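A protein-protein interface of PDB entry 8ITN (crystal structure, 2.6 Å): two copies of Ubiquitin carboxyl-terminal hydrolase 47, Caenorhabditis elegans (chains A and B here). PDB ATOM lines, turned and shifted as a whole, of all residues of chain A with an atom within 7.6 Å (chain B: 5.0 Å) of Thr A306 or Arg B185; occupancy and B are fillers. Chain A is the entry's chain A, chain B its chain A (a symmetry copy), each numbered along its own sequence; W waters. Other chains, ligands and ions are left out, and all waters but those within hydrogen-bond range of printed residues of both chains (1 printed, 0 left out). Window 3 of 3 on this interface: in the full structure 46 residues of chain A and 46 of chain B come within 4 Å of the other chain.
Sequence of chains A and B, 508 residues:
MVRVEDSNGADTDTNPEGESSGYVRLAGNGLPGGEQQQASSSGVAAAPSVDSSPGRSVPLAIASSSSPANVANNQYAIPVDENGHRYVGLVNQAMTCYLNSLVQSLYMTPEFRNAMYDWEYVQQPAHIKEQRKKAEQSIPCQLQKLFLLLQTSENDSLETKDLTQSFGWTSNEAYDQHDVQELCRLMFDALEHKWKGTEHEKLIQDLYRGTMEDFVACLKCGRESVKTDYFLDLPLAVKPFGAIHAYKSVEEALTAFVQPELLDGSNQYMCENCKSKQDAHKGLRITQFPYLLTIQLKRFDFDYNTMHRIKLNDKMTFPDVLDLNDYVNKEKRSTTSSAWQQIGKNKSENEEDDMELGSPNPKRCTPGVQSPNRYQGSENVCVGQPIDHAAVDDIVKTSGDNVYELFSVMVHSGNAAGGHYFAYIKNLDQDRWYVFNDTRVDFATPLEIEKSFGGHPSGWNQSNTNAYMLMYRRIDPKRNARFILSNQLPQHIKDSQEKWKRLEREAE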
ATOM      1  N   ASP A 301     -41.373 -25.403 -21.273  1.00  0.00           N
ATOM      2  CA  ASP A 301     -40.165 -24.943 -20.610  1.00  0.00           C
ATOM      3  C   ASP A 301     -39.082 -24.769 -21.664  1.00  0.00           C
ATOM      4  O   ASP A 301     -39.211 -25.238 -22.799  1.00  0.00           O
ATOM      5  CB  ASP A 301     -39.718 -25.931 -19.524  1.00  0.00           C
ATOM      6  CG  ASP A 301     -38.925 -25.264 -18.417  1.00  0.00           C
ATOM      7  OD1 ASP A 301     -38.754 -24.027 -18.467  1.00  0.00           O
ATOM      8  OD2 ASP A 301     -38.478 -25.979 -17.495  1.00  0.00           O
ATOM      9  N   PHE A 302     -38.005 -24.080 -21.300  1.00  0.00           N
ATOM     10  CA  PHE A 302     -36.884 -23.875 -22.211  1.00  0.00           C
ATOM     11  C   PHE A 302     -35.657 -24.577 -21.646  1.00  0.00           C
ATOM     12  O   PHE A 302     -35.125 -24.172 -20.607  1.00  0.00           O
ATOM     13  CB  PHE A 302     -36.604 -22.391 -22.442  1.00  0.00           C
ATOM     14  CG  PHE A 302     -35.643 -22.134 -23.570  1.00  0.00           C
ATOM     15  CD1 PHE A 302     -36.097 -22.029 -24.874  1.00  0.00           C
ATOM     16  CD2 PHE A 302     -34.284 -22.018 -23.328  1.00  0.00           C
ATOM     17  CE1 PHE A 302     -35.216 -21.801 -25.916  1.00  0.00           C
ATOM     18  CE2 PHE A 302     -33.397 -21.790 -24.366  1.00  0.00           C
ATOM     19  CZ  PHE A 302     -33.864 -21.682 -25.661  1.00  0.00           C
ATOM     20  N   ASP A 303     -35.215 -25.627 -22.331  1.00  0.00           N
ATOM     21  CA  ASP A 303     -33.967 -26.297 -21.995  1.00  0.00           C
ATOM     22  C   ASP A 303     -32.810 -25.483 -22.561  1.00  0.00           C
ATOM     23  O   ASP A 303     -32.758 -25.228 -23.768  1.00  0.00           O
ATOM     24  CB  ASP A 303     -33.963 -27.718 -22.555  1.00  0.00           C
ATOM     25  CG  ASP A 303     -32.793 -28.547 -22.055  1.00  0.00           C
ATOM     26  OD1 ASP A 303     -32.015 -28.047 -21.215  1.00  0.00           O
ATOM     27  OD2 ASP A 303     -32.654 -29.705 -22.502  1.00  0.00           O
ATOM     28  N   TYR A 304     -31.891 -25.061 -21.692  1.00  0.00           N
ATOM     29  CA  TYR A 304     -30.729 -24.306 -22.140  1.00  0.00           C
ATOM     30  C   TYR A 304     -29.614 -25.195 -22.673  1.00  0.00           C
ATOM     31  O   TYR A 304     -28.650 -24.675 -23.246  1.00  0.00           O
ATOM     32  CB  TYR A 304     -30.190 -23.436 -21.001  1.00  0.00           C
ATOM     33  CG  TYR A 304     -31.066 -22.248 -20.670  1.00  0.00           C
ATOM     34  CD1 TYR A 304     -30.927 -21.048 -21.355  1.00  0.00           C
ATOM     35  CD2 TYR A 304     -32.029 -22.325 -19.672  1.00  0.00           C
ATOM     36  CE1 TYR A 304     -31.721 -19.958 -21.058  1.00  0.00           C
ATOM     37  CE2 TYR A 304     -32.830 -21.239 -19.366  1.00  0.00           C
ATOM     38  CZ  TYR A 304     -32.671 -20.058 -20.063  1.00  0.00           C
ATOM     39  OH  TYR A 304     -33.466 -18.975 -19.762  1.00  0.00           O
ATOM     40  N   ASN A 305     -29.730 -26.512 -22.516  1.00  0.00           N
ATOM     41  CA  ASN A 305     -28.688 -27.432 -22.986  1.00  0.00           C
ATOM     42  C   ASN A 305     -28.923 -27.959 -24.406  1.00  0.00           C
ATOM     43  O   ASN A 305     -28.057 -28.599 -25.001  1.00  0.00           O
ATOM     44  CB  ASN A 305     -28.531 -28.603 -22.013  1.00  0.00           C
ATOM     45  CG  ASN A 305     -28.457 -28.153 -20.567  1.00  0.00           C
ATOM     46  OD1 ASN A 305     -27.658 -27.285 -20.214  1.00  0.00           O
ATOM     47  ND2 ASN A 305     -29.293 -28.743 -19.721  1.00  0.00           N
ATOM     48  N   THR A 306     -30.109 -27.674 -24.927  1.00  0.00           N
ATOM     49  CA  THR A 306     -30.551 -28.082 -26.246  1.00  0.00           C
ATOM     50  C   THR A 306     -29.963 -27.191 -27.322  1.00  0.00           C
ATOM     51  O   THR A 306     -29.192 -27.672 -28.153  1.00  0.00           O
ATOM     52  CB  THR A 306     -32.087 -28.057 -26.358  1.00  0.00           C
ATOM     53  OG1 THR A 306     -32.637 -27.311 -25.265  1.00  0.00           O
ATOM     54  CG2 THR A 306     -32.646 -29.470 -26.334  1.00  0.00           C
ATOM     55  N   MET A 307     -30.301 -25.901 -27.341  1.00  0.00           N
ATOM     56  CA  MET A 307     -31.191 -25.188 -26.428  1.00  0.00           C
ATOM     57  C   MET A 307     -32.511 -24.849 -27.121  1.00  0.00           C
ATOM     58  O   MET A 307     -32.647 -23.803 -27.757  1.00  0.00           O
ATOM     59  CB  MET A 307     -30.518 -23.919 -25.893  1.00  0.00           C
ATOM     60  CG  MET A 307     -29.692 -23.153 -26.916  1.00  0.00           C
ATOM     61  SD  MET A 307     -28.857 -21.722 -26.202  1.00  0.00           S
ATOM     62  CE  MET A 307     -30.252 -20.732 -25.674  1.00  0.00           C
ATOM     63  N   HIS A 308     -33.480 -25.751 -26.993  1.00  0.00           N
ATOM     64  CA  HIS A 308     -34.787 -25.615 -27.617  1.00  0.00           C
ATOM     65  C   HIS A 308     -35.880 -25.669 -26.556  1.00  0.00           C
ATOM     66  O   HIS A 308     -35.631 -25.946 -25.380  1.00  0.00           O
ATOM     67  CB  HIS A 308     -35.023 -26.715 -28.662  1.00  0.00           C
ATOM     68  CG  HIS A 308     -34.064 -26.682 -29.810  1.00  0.00           C
ATOM     69  ND1 HIS A 308     -32.727 -26.988 -29.674  1.00  0.00           N
ATOM     70  CD2 HIS A 308     -34.251 -26.391 -31.119  1.00  0.00           C
ATOM     71  CE1 HIS A 308     -32.131 -26.881 -30.848  1.00  0.00           C
ATOM     72  NE2 HIS A 308     -33.033 -26.519 -31.742  1.00  0.00           N
ATOM     73  N   ARG A 309     -37.107 -25.406 -26.995  1.00  0.00           N
ATOM     74  CA  ARG A 309     -38.262 -25.545 -26.120  1.00  0.00           C
ATOM     75  C   ARG A 309     -38.582 -27.019 -25.892  1.00  0.00           C
ATOM     76  O   ARG A 309     -38.376 -27.866 -26.764  1.00  0.00           O
ATOM     77  CB  ARG A 309     -39.478 -24.835 -26.719  1.00  0.00           C
ATOM     78  CG  ARG A 309     -39.462 -23.318 -26.594  1.00  0.00           C
ATOM     79  CD  ARG A 309     -40.662 -22.699 -27.304  1.00  0.00           C
ATOM     80  NE  ARG A 309     -40.845 -21.293 -26.963  1.00  0.00           N
ATOM     81  CZ  ARG A 309     -41.751 -20.499 -27.517  1.00  0.00           C
ATOM     82  NH1 ARG A 309     -42.567 -20.934 -28.463  1.00  0.00           N
ATOM     83  NH2 ARG A 309     -41.842 -19.235 -27.111  1.00  0.00           N
ATOM     84  N   ILE A 310     -39.084 -27.320 -24.694  1.00  0.00           N
ATOM     85  CA  ILE A 310     -39.569 -28.648 -24.345  1.00  0.00           C
ATOM     86  C   ILE A 310     -40.973 -28.499 -23.778  1.00  0.00           C
ATOM     87  O   ILE A 310     -41.394 -27.412 -23.377  1.00  0.00           O
ATOM     88  CB  ILE A 310     -38.648 -29.372 -23.340  1.00  0.00           C
ATOM     89  CG1 ILE A 310     -38.535 -28.570 -22.043  1.00  0.00           C
ATOM     90  CG2 ILE A 310     -37.273 -29.615 -23.952  1.00  0.00           C
ATOM     91  CD1 ILE A 310     -37.680 -29.236 -20.986  1.00  0.00           C
ATOM     92  N   GLN B 181     -26.793 -18.368 -18.577  1.00  0.00           N
ATOM     93  CA  GLN B 181     -26.581 -19.593 -19.340  1.00  0.00           C
ATOM     94  C   GLN B 181     -26.543 -19.319 -20.836  1.00  0.00           C
ATOM     95  O   GLN B 181     -25.843 -20.019 -21.577  1.00  0.00           O
ATOM     96  CB  GLN B 181     -27.675 -20.605 -19.006  1.00  0.00           C
ATOM     97  CG  GLN B 181     -28.083 -20.591 -17.541  1.00  0.00           C
ATOM     98  CD  GLN B 181     -29.174 -21.593 -17.224  1.00  0.00           C
ATOM     99  OE1 GLN B 181     -29.124 -22.744 -17.659  1.00  0.00           O
ATOM    100  NE2 GLN B 181     -30.172 -21.158 -16.463  1.00  0.00           N
ATOM    101  N   GLU B 182     -27.284 -18.309 -21.299  1.00  0.00           N
ATOM    102  CA  GLU B 182     -27.226 -17.943 -22.710  1.00  0.00           C
ATOM    103  C   GLU B 182     -25.870 -17.347 -23.068  1.00  0.00           C
ATOM    104  O   GLU B 182     -25.342 -17.599 -24.157  1.00  0.00           O
ATOM    105  CB  GLU B 182     -28.347 -16.962 -23.052  1.00  0.00           C
ATOM    106  CG  GLU B 182     -29.743 -17.475 -22.752  1.00  0.00           C
ATOM    107  CD  GLU B 182     -30.821 -16.635 -23.410  1.00  0.00           C
ATOM    108  OE1 GLU B 182     -30.569 -16.097 -24.509  1.00  0.00           O
ATOM    109  OE2 GLU B 182     -31.919 -16.511 -22.828  1.00  0.00           O
ATOM    110  N   LEU B 183     -25.293 -16.552 -22.163  1.00  0.00           N
ATOM    111  CA  LEU B 183     -23.978 -15.975 -22.423  1.00  0.00           C
ATOM    112  C   LEU B 183     -22.893 -17.044 -22.404  1.00  0.00           C
ATOM    113  O   LEU B 183     -21.962 -17.004 -23.216  1.00  0.00           O
ATOM    114  CB  LEU B 183     -23.677 -14.878 -21.401  1.00  0.00           C
ATOM    115  CG  LEU B 183     -22.359 -14.123 -21.587  1.00  0.00           C
ATOM    116  CD1 LEU B 183     -22.279 -13.525 -22.982  1.00  0.00           C
ATOM    117  CD2 LEU B 183     -22.202 -13.041 -20.530  1.00  0.00           C
ATOM    118  N   CYS B 184     -22.998 -18.008 -21.484  1.00  0.00           N
ATOM    119  CA  CYS B 184     -22.055 -19.123 -21.470  1.00  0.00           C
ATOM    120  C   CYS B 184     -22.126 -19.915 -22.768  1.00  0.00           C
ATOM    121  O   CYS B 184     -21.098 -20.350 -23.298  1.00  0.00           O
ATOM    122  CB  CYS B 184     -22.334 -20.036 -20.277  1.00  0.00           C
ATOM    123  SG  CYS B 184     -22.147 -19.254 -18.665  1.00  0.00           S
ATOM    124  N   ARG B 185     -23.337 -20.108 -23.297  1.00  0.00           N
ATOM    125  CA  ARG B 185     -23.488 -20.851 -24.543  1.00  0.00           C
ATOM    126  C   ARG B 185     -22.939 -20.064 -25.727  1.00  0.00           C
ATOM    127  O   ARG B 185     -22.339 -20.643 -26.638  1.00  0.00           O
ATOM    128  CB  ARG B 185     -24.958 -21.207 -24.763  1.00  0.00           C
ATOM    129  CG  ARG B 185     -25.202 -22.101 -25.965  1.00  0.00           C
ATOM    130  CD  ARG B 185     -24.342 -23.351 -25.895  1.00  0.00           C
ATOM    131  NE  ARG B 185     -25.140 -24.568 -25.953  1.00  0.00           N
ATOM    132  CZ  ARG B 185     -25.492 -25.179 -27.076  1.00  0.00           C
ATOM    133  NH1 ARG B 185     -25.137 -24.706 -28.260  1.00  0.00           N
ATOM    134  NH2 ARG B 185     -26.216 -26.293 -27.010  1.00  0.00           N
ATOM    135  N   LEU B 186     -23.131 -18.742 -25.729  1.00  0.00           N
ATOM    136  CA  LEU B 186     -22.609 -17.925 -26.820  1.00  0.00           C
ATOM    137  C   LEU B 186     -21.086 -17.950 -26.847  1.00  0.00           C
ATOM    138  O   LEU B 186     -20.475 -18.041 -27.918  1.00  0.00           O
ATOM    139  CB  LEU B 186     -23.119 -16.489 -26.690  1.00  0.00           C
ATOM    140  CG  LEU B 186     -22.820 -15.569 -27.876  1.00  0.00           C
ATOM    141  CD1 LEU B 186     -23.880 -15.722 -28.956  1.00  0.00           C
ATOM    142  CD2 LEU B 186     -22.694 -14.121 -27.429  1.00  0.00           C
ATOM    143  N   MET B 187     -20.455 -17.869 -25.674  1.00  0.00           N
ATOM    144  CA  MET B 187     -18.998 -17.909 -25.620  1.00  0.00           C
ATOM    145  C   MET B 187     -18.470 -19.289 -25.997  1.00  0.00           C
ATOM    146  O   MET B 187     -17.479 -19.402 -26.727  1.00  0.00           O
ATOM    147  CB  MET B 187     -18.511 -17.509 -24.227  1.00  0.00           C
ATOM    148  CG  MET B 187     -18.904 -16.100 -23.812  1.00  0.00           C
ATOM    149  SD  MET B 187     -18.430 -15.721 -22.113  1.00  0.00           S
ATOM    150  CE  MET B 187     -16.656 -15.927 -22.211  1.00  0.00           C
ATOM    151  N   PHE B 188     -19.122 -20.348 -25.514  1.00  0.00           N
ATOM    152  CA  PHE B 188     -18.660 -21.699 -25.816  1.00  0.00           C
ATOM    153  C   PHE B 188     -18.880 -22.053 -27.282  1.00  0.00           C
ATOM    154  O   PHE B 188     -18.074 -22.788 -27.864  1.00  0.00           O
ATOM    155  CB  PHE B 188     -19.357 -22.718 -24.910  1.00  0.00           C
ATOM    156  CG  PHE B 188     -18.848 -22.725 -23.495  1.00  0.00           C
ATOM    157  CD1 PHE B 188     -17.835 -21.865 -23.099  1.00  0.00           C
ATOM    158  CD2 PHE B 188     -19.374 -23.605 -22.564  1.00  0.00           C
ATOM    159  CE1 PHE B 188     -17.366 -21.876 -21.799  1.00  0.00           C
ATOM    160  CE2 PHE B 188     -18.906 -23.620 -21.262  1.00  0.00           C
ATOM    161  CZ  PHE B 188     -17.903 -22.756 -20.882  1.00  0.00           C
ATOM    162  N   ASP B 189     -19.955 -21.548 -27.892  1.00  0.00           N
ATOM    163  CA  ASP B 189     -20.181 -21.811 -29.310  1.00  0.00           C
ATOM    164  C   ASP B 189     -19.108 -21.155 -30.169  1.00  0.00           C
ATOM    165  O   ASP B 189     -18.624 -21.753 -31.137  1.00  0.00           O
ATOM    166  CB  ASP B 189     -21.568 -21.321 -29.726  1.00  0.00           C
ATOM    167  CG  ASP B 189     -22.684 -22.191 -29.182  1.00  0.00           C
ATOM    168  OD1 ASP B 189     -22.430 -23.378 -28.885  1.00  0.00           O
ATOM    169  OD2 ASP B 189     -23.819 -21.688 -29.057  1.00  0.00           O
ATOM    170  N   ALA B 190     -18.720 -19.925 -29.825  1.00  0.00           N
ATOM    171  CA  ALA B 190     -17.684 -19.229 -30.580  1.00  0.00           C
ATOM    172  C   ALA B 190     -16.331 -19.906 -30.412  1.00  0.00           C
ATOM    173  O   ALA B 190     -15.572 -20.036 -31.379  1.00  0.00           O
ATOM    174  CB  ALA B 190     -17.611 -17.769 -30.142  1.00  0.00           C
ATOM    175  N   LEU B 232     -24.863 -29.140 -20.112  1.00  0.00           N
ATOM    176  CA  LEU B 232     -23.790 -28.277 -19.642  1.00  0.00           C
ATOM    177  C   LEU B 232     -24.108 -27.616 -18.309  1.00  0.00           C
ATOM    178  O   LEU B 232     -23.224 -26.979 -17.726  1.00  0.00           O
ATOM    179  CB  LEU B 232     -23.479 -27.189 -20.683  1.00  0.00           C
ATOM    180  CG  LEU B 232     -22.571 -27.528 -21.870  1.00  0.00           C
ATOM    181  CD1 LEU B 232     -23.206 -28.552 -22.802  1.00  0.00           C
ATOM    182  CD2 LEU B 232     -22.211 -26.262 -22.632  1.00  0.00           C
HETATM  183  O   HOH W   1     -26.943 -18.753 -25.887  1.00  0.00           O
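OD1 of Asp A303 sits at hydrogen-bond distance from N of Asn A305.
The backbone carbonyl oxygen (O) of Asp A303 is in hydrogen-bond range of the side-chain hydroxyl (OG1) of Thr A306.
The side-chain hydroxyl (OG1) of Thr A306 is in hydrogen-bond range of the backbone NH (N) of His A308, 2.5 Å away.
NH1 of Arg B185 is in salt-bridge range of OD1 of Asp B189 (3.1 Å).
Gln B181 touches Tyr A304 (OE1 to CD2, 3.6 Å).
Glu B182 touches Tyr A304 (CG to CE1, 3.6 Å).
O of Asn A305 touches NH2 of Arg B185, at 3.6 Å.
SD of Met A307 touches CG of Arg B185 (3.7 Å).
OD1 of Asn A305 lies within hydrogen-bond range of N of Leu B232, at 3.4 Å.
The backbone carbonyl oxygen (O) of Thr A306 lies within hydrogen-bond range of the guanidinium group (NH2) of Arg B185, 3.5 Å away.
Of the printed residues of chain B, Tyr A304 touches Gln B181 (3.6 Å) and Glu B182 (3.6 Å).
Printed residues of chain A within 4 Å of Gln B181: Tyr A304 (3.6 Å).
The nearest printed residue of chain A that does not touch Glu B182 is Met A307 (4.4 Å).
No position is printed for both chains.
Of the 6 pairs that touch across the chains among the printed residues, none has its exchanged pair printed and touching as well.
Water W1 lies within hydrogen-bond range of O of Glu B182 (2.6 Å) and SD of Met A307 (3.5 Å).
Printed residues of chain B that touch a printed residue of chain A: Gln B181, Glu B182, Arg B185 and Leu B232.
Of the 10 printed residues of chain A, 4 touch a printed residue of chain B.
Hydrophobic or aromatic side chains of chain A within 4 Å of the printed part of chain B: Tyr A304 and Met A307.
Among the printed residues, 6 pairs touch across the chains.
Among the printed residues, no Asp or Glu carboxylate lies within 4 Å of a Lys or Arg side-chain nitrogen of the other chain.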
